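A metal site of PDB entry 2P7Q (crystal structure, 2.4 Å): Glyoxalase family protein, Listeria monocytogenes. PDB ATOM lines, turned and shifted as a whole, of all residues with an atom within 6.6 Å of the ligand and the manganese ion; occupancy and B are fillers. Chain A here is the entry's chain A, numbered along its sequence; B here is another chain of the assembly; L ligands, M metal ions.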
ATOM      1  N   TYR A  67     -13.269  -0.432 -17.670  1.00  0.00           N
ATOM      2  CA  TYR A  67     -12.893  -1.483 -18.589  1.00  0.00           C
ATOM      3  C   TYR A  67     -14.078  -2.322 -19.002  1.00  0.00           C
ATOM      4  O   TYR A  67     -13.940  -3.270 -19.757  1.00  0.00           O
ATOM      5  CB  TYR A  67     -11.804  -2.367 -17.992  1.00  0.00           C
ATOM      6  CG  TYR A  67     -11.178  -3.319 -18.989  1.00  0.00           C
ATOM      7  CD1 TYR A  67     -10.750  -2.869 -20.238  1.00  0.00           C
ATOM      8  CD2 TYR A  67     -11.033  -4.676 -18.686  1.00  0.00           C
ATOM      9  CE1 TYR A  67     -10.199  -3.759 -21.172  1.00  0.00           C
ATOM     10  CE2 TYR A  67     -10.489  -5.572 -19.615  1.00  0.00           C
ATOM     11  CZ  TYR A  67     -10.075  -5.111 -20.848  1.00  0.00           C
ATOM     12  OH  TYR A  67      -9.567  -5.997 -21.774  1.00  0.00           O
ATOM     13  N   HIS A  69     -16.750  -3.415 -21.237  1.00  0.00           N
ATOM     14  CA  HIS A  69     -16.877  -3.178 -22.672  1.00  0.00           C
ATOM     15  C   HIS A  69     -17.683  -4.223 -23.429  1.00  0.00           C
ATOM     16  O   HIS A  69     -17.971  -5.314 -22.944  1.00  0.00           O
ATOM     17  CB  HIS A  69     -15.485  -3.047 -23.334  1.00  0.00           C
ATOM     18  CG  HIS A  69     -14.606  -4.257 -23.189  1.00  0.00           C
ATOM     19  ND1 HIS A  69     -13.782  -4.443 -22.105  1.00  0.00           N
ATOM     20  CD2 HIS A  69     -14.392  -5.307 -24.014  1.00  0.00           C
ATOM     21  CE1 HIS A  69     -13.094  -5.560 -22.266  1.00  0.00           C
ATOM     22  NE2 HIS A  69     -13.442  -6.101 -23.416  1.00  0.00           N
ATOM     23  N   ILE A  70     -18.065  -3.843 -24.645  1.00  0.00           N
ATOM     24  CA  ILE A  70     -18.818  -4.710 -25.536  1.00  0.00           C
ATOM     25  C   ILE A  70     -17.830  -4.985 -26.646  1.00  0.00           C
ATOM     26  O   ILE A  70     -17.062  -4.104 -27.027  1.00  0.00           O
ATOM     27  CB  ILE A  70     -20.046  -3.989 -26.089  1.00  0.00           C
ATOM     28  CG1 ILE A  70     -20.836  -3.370 -24.931  1.00  0.00           C
ATOM     29  CG2 ILE A  70     -20.942  -4.957 -26.833  1.00  0.00           C
ATOM     30  CD1 ILE A  70     -22.124  -2.699 -25.348  1.00  0.00           C
ATOM     31  N   ALA A  71     -17.810  -6.202 -27.149  1.00  0.00           N
ATOM     32  CA  ALA A  71     -16.844  -6.562 -28.183  1.00  0.00           C
ATOM     33  C   ALA A  71     -17.497  -7.221 -29.369  1.00  0.00           C
ATOM     34  O   ALA A  71     -18.262  -8.169 -29.215  1.00  0.00           O
ATOM     35  CB  ALA A  71     -15.788  -7.479 -27.613  1.00  0.00           C
ATOM     36  N   ARG A  97      -3.170  -3.579 -26.232  1.00  0.00           N
ATOM     37  CA  ARG A  97      -3.205  -4.206 -24.920  1.00  0.00           C
ATOM     38  C   ARG A  97      -2.303  -5.456 -24.933  1.00  0.00           C
ATOM     39  O   ARG A  97      -2.230  -6.158 -25.955  1.00  0.00           O
ATOM     40  CB  ARG A  97      -4.649  -4.569 -24.612  1.00  0.00           C
ATOM     41  CG  ARG A  97      -4.951  -4.860 -23.178  1.00  0.00           C
ATOM     42  CD  ARG A  97      -6.421  -5.136 -23.000  1.00  0.00           C
ATOM     43  NE  ARG A  97      -6.754  -5.390 -21.608  1.00  0.00           N
ATOM     44  CZ  ARG A  97      -6.698  -4.463 -20.653  1.00  0.00           C
ATOM     45  NH1 ARG A  97      -6.326  -3.232 -20.952  1.00  0.00           N
ATOM     46  NH2 ARG A  97      -6.999  -4.790 -19.405  1.00  0.00           N
ATOM     47  N   PRO A  98      -1.614  -5.753 -23.819  1.00  0.00           N
ATOM     48  CA  PRO A  98      -0.729  -6.936 -23.745  1.00  0.00           C
ATOM     49  C   PRO A  98      -1.461  -8.246 -24.018  1.00  0.00           C
ATOM     50  O   PRO A  98      -2.460  -8.546 -23.375  1.00  0.00           O
ATOM     51  CB  PRO A  98      -0.175  -6.864 -22.327  1.00  0.00           C
ATOM     52  CG  PRO A  98      -0.175  -5.394 -22.043  1.00  0.00           C
ATOM     53  CD  PRO A  98      -1.514  -4.957 -22.585  1.00  0.00           C
ATOM     54  N   ARG A  99      -0.938  -9.023 -24.977  1.00  0.00           N
ATOM     55  CA  ARG A  99      -1.523 -10.301 -25.370  1.00  0.00           C
ATOM     56  C   ARG A  99      -0.831 -11.532 -24.762  1.00  0.00           C
ATOM     57  O   ARG A  99      -0.013 -11.407 -23.854  1.00  0.00           O
ATOM     58  CB  ARG A  99      -1.493 -10.441 -26.900  1.00  0.00           C
ATOM     59  CG  ARG A  99      -2.596  -9.685 -27.627  1.00  0.00           C
ATOM     60  CD  ARG A  99      -2.349  -9.666 -29.132  1.00  0.00           C
ATOM     61  NE  ARG A  99      -1.279  -8.749 -29.502  1.00  0.00           N
ATOM     62  CZ  ARG A  99      -0.773  -8.647 -30.720  1.00  0.00           C
ATOM     63  NH1 ARG A  99      -1.229  -9.407 -31.694  1.00  0.00           N
ATOM     64  NH2 ARG A  99       0.208  -7.770 -30.962  1.00  0.00           N
ATOM     65  N   GLU A 103      -3.766 -15.030 -28.567  1.00  0.00           N
ATOM     66  CA  GLU A 103      -4.859 -14.116 -28.278  1.00  0.00           C
ATOM     67  C   GLU A 103      -4.856 -13.186 -29.496  1.00  0.00           C
ATOM     68  O   GLU A 103      -3.871 -12.490 -29.751  1.00  0.00           O
ATOM     69  CB  GLU A 103      -4.545 -13.340 -26.994  1.00  0.00           C
ATOM     70  CG  GLU A 103      -5.657 -12.458 -26.431  1.00  0.00           C
ATOM     71  CD  GLU A 103      -5.290 -11.855 -25.075  1.00  0.00           C
ATOM     72  OE1 GLU A 103      -6.078 -11.058 -24.521  1.00  0.00           O
ATOM     73  OE2 GLU A 103      -4.199 -12.187 -24.561  1.00  0.00           O
ATOM     74  N   GLY A 104      -5.950 -13.201 -30.261  1.00  0.00           N
ATOM     75  CA  GLY A 104      -6.025 -12.379 -31.450  1.00  0.00           C
ATOM     76  C   GLY A 104      -5.892 -10.885 -31.204  1.00  0.00           C
ATOM     77  O   GLY A 104      -6.049 -10.420 -30.066  1.00  0.00           O
ATOM     78  N   SER A 106      -6.780  -6.878 -31.150  1.00  0.00           N
ATOM     79  CA  SER A 106      -7.998  -6.143 -30.793  1.00  0.00           C
ATOM     80  C   SER A 106      -7.819  -4.636 -31.009  1.00  0.00           C
ATOM     81  O   SER A 106      -6.701  -4.124 -31.015  1.00  0.00           O
ATOM     82  CB  SER A 106      -8.353  -6.366 -29.325  1.00  0.00           C
ATOM     83  OG  SER A 106      -8.712  -7.707 -29.041  1.00  0.00           O
ATOM     84  N   TYR A 108      -9.458  -1.104 -29.410  1.00  0.00           N
ATOM     85  CA  TYR A 108     -10.329  -0.541 -28.389  1.00  0.00           C
ATOM     86  C   TYR A 108     -10.517   0.941 -28.677  1.00  0.00           C
ATOM     87  O   TYR A 108      -9.602   1.594 -29.191  1.00  0.00           O
ATOM     88  CB  TYR A 108      -9.723  -0.739 -26.989  1.00  0.00           C
ATOM     89  CG  TYR A 108      -9.979  -2.120 -26.394  1.00  0.00           C
ATOM     90  CD1 TYR A 108      -8.993  -3.114 -26.385  1.00  0.00           C
ATOM     91  CD2 TYR A 108     -11.213  -2.412 -25.804  1.00  0.00           C
ATOM     92  CE1 TYR A 108      -9.235  -4.361 -25.791  1.00  0.00           C
ATOM     93  CE2 TYR A 108     -11.456  -3.659 -25.210  1.00  0.00           C
ATOM     94  CZ  TYR A 108     -10.471  -4.625 -25.210  1.00  0.00           C
ATOM     95  OH  TYR A 108     -10.736  -5.838 -24.605  1.00  0.00           O
ATOM     96  N   GLU A 118     -14.926  -2.491 -28.656  1.00  0.00           N
ATOM     97  CA  GLU A 118     -13.811  -3.289 -29.121  1.00  0.00           C
ATOM     98  C   GLU A 118     -14.173  -4.100 -30.342  1.00  0.00           C
ATOM     99  O   GLU A 118     -15.275  -4.627 -30.450  1.00  0.00           O
ATOM    100  CB  GLU A 118     -13.325  -4.241 -28.030  1.00  0.00           C
ATOM    101  CG  GLU A 118     -12.494  -5.412 -28.573  1.00  0.00           C
ATOM    102  CD  GLU A 118     -12.097  -6.398 -27.485  1.00  0.00           C
ATOM    103  OE1 GLU A 118     -12.891  -6.558 -26.537  1.00  0.00           O
ATOM    104  OE2 GLU A 118     -11.013  -7.016 -27.609  1.00  0.00           O
ATOM    105  N   HIS A 120     -12.781  -7.269 -31.914  1.00  0.00           N
ATOM    106  CA  HIS A 120     -11.892  -8.392 -31.634  1.00  0.00           C
ATOM    107  C   HIS A 120     -11.714  -9.343 -32.814  1.00  0.00           C
ATOM    108  O   HIS A 120     -12.671  -9.733 -33.475  1.00  0.00           O
ATOM    109  CB  HIS A 120     -12.436  -9.169 -30.417  1.00  0.00           C
ATOM    110  CG  HIS A 120     -11.546 -10.290 -29.949  1.00  0.00           C
ATOM    111  ND1 HIS A 120     -10.245 -10.092 -29.531  1.00  0.00           N
ATOM    112  CD2 HIS A 120     -11.800 -11.606 -29.769  1.00  0.00           C
ATOM    113  CE1 HIS A 120      -9.737 -11.237 -29.110  1.00  0.00           C
ATOM    114  NE2 HIS A 120     -10.660 -12.172 -29.251  1.00  0.00           N
ATOM    115  N   ARG A 127      -8.527 -19.239 -27.334  1.00  0.00           N
ATOM    116  CA  ARG A 127      -8.283 -18.708 -25.991  1.00  0.00           C
ATOM    117  C   ARG A 127      -8.513 -19.760 -24.902  1.00  0.00           C
ATOM    118  O   ARG A 127      -8.333 -19.488 -23.717  1.00  0.00           O
ATOM    119  CB  ARG A 127      -9.210 -17.509 -25.763  1.00  0.00           C
ATOM    120  CG  ARG A 127      -9.008 -16.751 -24.470  1.00  0.00           C
ATOM    121  CD  ARG A 127      -7.620 -16.133 -24.396  1.00  0.00           C
ATOM    122  NE  ARG A 127      -7.571 -15.077 -23.388  1.00  0.00           N
ATOM    123  CZ  ARG A 127      -8.138 -13.884 -23.533  1.00  0.00           C
ATOM    124  NH1 ARG A 127      -8.792 -13.579 -24.651  1.00  0.00           N
ATOM    125  NH2 ARG A 127      -8.052 -12.989 -22.551  1.00  0.00           N
ATOM    126  N   HIS B   7     -18.071 -10.795 -27.418  1.00  0.00           N
ATOM    127  CA  HIS B   7     -18.259 -10.987 -25.993  1.00  0.00           C
ATOM    128  C   HIS B   7     -18.488  -9.685 -25.235  1.00  0.00           C
ATOM    129  O   HIS B   7     -18.257  -8.599 -25.770  1.00  0.00           O
ATOM    130  CB  HIS B   7     -17.034 -11.654 -25.392  1.00  0.00           C
ATOM    131  CG  HIS B   7     -15.786 -10.839 -25.514  1.00  0.00           C
ATOM    132  ND1 HIS B   7     -14.936 -10.930 -26.607  1.00  0.00           N
ATOM    133  CD2 HIS B   7     -15.250  -9.900 -24.698  1.00  0.00           C
ATOM    134  CE1 HIS B   7     -13.929 -10.088 -26.442  1.00  0.00           C
ATOM    135  NE2 HIS B   7     -14.103  -9.451 -25.299  1.00  0.00           N
ATOM    136  N   ILE B   8     -18.936  -9.801 -23.992  1.00  0.00           N
ATOM    137  CA  ILE B   8     -19.170  -8.646 -23.122  1.00  0.00           C
ATOM    138  C   ILE B   8     -18.324  -8.846 -21.862  1.00  0.00           C
ATOM    139  O   ILE B   8     -18.387  -9.895 -21.223  1.00  0.00           O
ATOM    140  CB  ILE B   8     -20.641  -8.536 -22.686  1.00  0.00           C
ATOM    141  CG1 ILE B   8     -21.553  -8.413 -23.903  1.00  0.00           C
ATOM    142  CG2 ILE B   8     -20.812  -7.362 -21.740  1.00  0.00           C
ATOM    143  CD1 ILE B   8     -23.018  -8.294 -23.537  1.00  0.00           C
ATOM    144  N   THR B   9     -17.532  -7.835 -21.495  1.00  0.00           N
ATOM    145  CA  THR B   9     -16.693  -7.918 -20.313  1.00  0.00           C
ATOM    146  C   THR B   9     -17.169  -6.976 -19.214  1.00  0.00           C
ATOM    147  O   THR B   9     -17.339  -5.786 -19.441  1.00  0.00           O
ATOM    148  CB  THR B   9     -15.241  -7.586 -20.673  1.00  0.00           C
ATOM    149  OG1 THR B   9     -14.700  -8.645 -21.465  1.00  0.00           O
ATOM    150  CG2 THR B   9     -14.403  -7.399 -19.419  1.00  0.00           C
ATOM    151  N   GLU B  44      -9.878 -13.425 -13.652  1.00  0.00           N
ATOM    152  CA  GLU B  44     -10.942 -13.341 -14.629  1.00  0.00           C
ATOM    153  C   GLU B  44     -11.579 -14.696 -14.839  1.00  0.00           C
ATOM    154  O   GLU B  44     -11.021 -15.725 -14.481  1.00  0.00           O
ATOM    155  CB  GLU B  44     -10.414 -12.796 -15.960  1.00  0.00           C
ATOM    156  CG  GLU B  44      -9.105 -13.408 -16.420  1.00  0.00           C
ATOM    157  CD  GLU B  44      -8.597 -12.752 -17.698  1.00  0.00           C
ATOM    158  OE1 GLU B  44      -7.454 -13.066 -18.117  1.00  0.00           O
ATOM    159  OE2 GLU B  44      -9.342 -11.939 -18.276  1.00  0.00           O
ATOM    160  N   PHE B  46     -14.583 -16.809 -17.641  1.00  0.00           N
ATOM    161  CA  PHE B  46     -15.365 -16.736 -18.864  1.00  0.00           C
ATOM    162  C   PHE B  46     -16.535 -17.673 -18.697  1.00  0.00           C
ATOM    163  O   PHE B  46     -16.337 -18.847 -18.405  1.00  0.00           O
ATOM    164  CB  PHE B  46     -14.557 -17.206 -20.085  1.00  0.00           C
ATOM    165  CG  PHE B  46     -13.339 -16.382 -20.402  1.00  0.00           C
ATOM    166  CD1 PHE B  46     -12.470 -16.787 -21.393  1.00  0.00           C
ATOM    167  CD2 PHE B  46     -13.059 -15.198 -19.711  1.00  0.00           C
ATOM    168  CE1 PHE B  46     -11.346 -16.038 -21.707  1.00  0.00           C
ATOM    169  CE2 PHE B  46     -11.936 -14.443 -20.017  1.00  0.00           C
ATOM    170  CZ  PHE B  46     -11.072 -14.866 -21.019  1.00  0.00           C
ATOM    171  N   TRP B  53     -20.603 -15.488 -25.068  1.00  0.00           N
ATOM    172  CA  TRP B  53     -19.376 -15.443 -24.308  1.00  0.00           C
ATOM    173  C   TRP B  53     -19.324 -14.222 -23.389  1.00  0.00           C
ATOM    174  O   TRP B  53     -19.251 -13.090 -23.851  1.00  0.00           O
ATOM    175  CB  TRP B  53     -18.185 -15.422 -25.272  1.00  0.00           C
ATOM    176  CG  TRP B  53     -16.842 -15.201 -24.618  1.00  0.00           C
ATOM    177  CD1 TRP B  53     -16.556 -15.263 -23.271  1.00  0.00           C
ATOM    178  CD2 TRP B  53     -15.610 -14.888 -25.274  1.00  0.00           C
ATOM    179  NE1 TRP B  53     -15.224 -15.020 -23.063  1.00  0.00           N
ATOM    180  CE2 TRP B  53     -14.613 -14.783 -24.280  1.00  0.00           C
ATOM    181  CE3 TRP B  53     -15.245 -14.693 -26.607  1.00  0.00           C
ATOM    182  CZ2 TRP B  53     -13.286 -14.485 -24.580  1.00  0.00           C
ATOM    183  CZ3 TRP B  53     -13.918 -14.395 -26.907  1.00  0.00           C
ATOM    184  CH2 TRP B  53     -12.963 -14.298 -25.896  1.00  0.00           C
ATOM    185  N   CYS B  55     -17.300 -12.384 -20.227  1.00  0.00           N
ATOM    186  CA  CYS B  55     -16.076 -12.310 -19.452  1.00  0.00           C
ATOM    187  C   CYS B  55     -16.250 -11.426 -18.220  1.00  0.00           C
ATOM    188  O   CYS B  55     -16.721 -10.288 -18.318  1.00  0.00           O
ATOM    189  CB  CYS B  55     -14.941 -11.791 -20.321  1.00  0.00           C
ATOM    190  SG  CYS B  55     -13.474 -11.257 -19.410  1.00  0.00           S
ATOM    191  N   MET B  57     -14.209  -9.759 -15.015  1.00  0.00           N
ATOM    192  CA  MET B  57     -12.871  -9.457 -14.511  1.00  0.00           C
ATOM    193  C   MET B  57     -13.007  -8.729 -13.183  1.00  0.00           C
ATOM    194  O   MET B  57     -13.982  -8.031 -12.939  1.00  0.00           O
ATOM    195  CB  MET B  57     -12.097  -8.607 -15.523  1.00  0.00           C
ATOM    196  CG  MET B  57     -10.605  -8.542 -15.247  1.00  0.00           C
ATOM    197  SD  MET B  57      -9.701  -7.511 -16.430  1.00  0.00           S
ATOM    198  CE  MET B  57      -9.520  -8.642 -17.762  1.00  0.00           C
HETATM  199  O1  LIG L   1     -10.546  -8.503 -25.238  1.00  0.00           O
HETATM  200  C1  LIG L   1      -9.973  -9.790 -24.845  1.00  0.00           C
HETATM  201  C2  LIG L   1      -8.679 -10.055 -25.699  1.00  0.00           C
HETATM  202  C3  LIG L   1      -9.611  -9.800 -23.309  1.00  0.00           C
HETATM  203  O2  LIG L   1      -8.634  -8.810 -23.008  1.00  0.00           O
HETATM  204  P1  LIG L   1     -11.012  -9.512 -22.263  1.00  0.00           P
HETATM  205  O3  LIG L   1     -12.104 -10.594 -22.524  1.00  0.00           O
HETATM  206  O4  LIG L   1     -10.570  -9.570 -20.901  1.00  0.00           O
HETATM  207  O5  LIG L   1     -11.643  -8.078 -22.544  1.00  0.00           O
HETATM  208 MN    MN M   1     -12.463  -7.907 -24.564  1.00  0.00          MN
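The side-chain hydroxyl (OH) of Tyr 67 lies within hydrogen-bond range of an oxygen (O2) of the ligand (3.2 Å).
The side-chain hydroxyl (OG1) of Thr 9 of chain B lies within hydrogen-bond range of an oxygen (O3) of the ligand, at 3.4 Å.
The side-chain sulfur of Cys 55 of chain B lies within hydrogen-bond range of an oxygen (O3) of the ligand, at 3.5 Å.
ND1 of His 69 lies within hydrogen-bond range of O of Tyr 67.
The backbone NH (N) of Thr 9 of chain B sits at hydrogen-bond distance from the backbone carbonyl oxygen (O) of His 69, at 2.9 Å.
O of His 7 of chain B sits at hydrogen-bond distance from N of Ala 71, 2.8 Å away.
N of Glu 118 sits at hydrogen-bond distance from O of Ile 70.
OH of Tyr 67 lies close to OH of Tyr 108.
OH of Tyr 67 sits at hydrogen-bond distance from NE of Arg 97 (2.9 Å).
OG1 of Thr 9 of chain B lies close to SG of Cys 55 of chain B.
N of Cys 55 of chain B sits at hydrogen-bond distance from O of Ile 8 of chain B, at 2.9 Å.
Merely in contact with the ligand: Glu 103 (3.0 Å), His 120 (3.8 Å), Arg 127 (3.6 Å), Glu 44 of chain B (3.7 Å) and Met 57 of chain B (3.4 Å).
Hydrophobic or aromatic side chains within 4 Å of the ligand: Tyr 67, His 69, Tyr 108, His 120, His 7 of chain B and Met 57 of chain B.
Within 4 Å of the ligand: Tyr 67, His 69, Glu 103, Tyr 108, Glu 118, His 120, Arg 127, His 7 of chain B, Thr 9 of chain B, Glu 44 of chain B, Cys 55 of chain B and Met 57 of chain B.
The nearest printed residue that does not touch the ligand is Ser 106 (4.1 Å).
Merely in contact with the manganese ion: Thr 9 of chain B (3.9 Å).
Five residues have an atom within 4 Å of the manganese ion: His 69, Tyr 108, Glu 118, His 7 of chain B and Thr 9 of chain B.
The nearest printed residue that does not touch the manganese ion is Tyr 67 (4.5 Å).
The manganese ion is bound by an oxygen (O1) of the ligand (2.1 Å), an oxygen (O5) of the ligand (2.2 Å), a ring nitrogen (NE2) of His 69 (2.4 Å), a ring nitrogen (NE2) of His 7 of chain B (2.4 Å), the side-chain carboxylate (OE1) of Glu 118 (2.4 Å) and the side-chain hydroxyl (OH) of Tyr 108 (2.7 Å).
The manganese ion has six donor atoms within binding distance.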
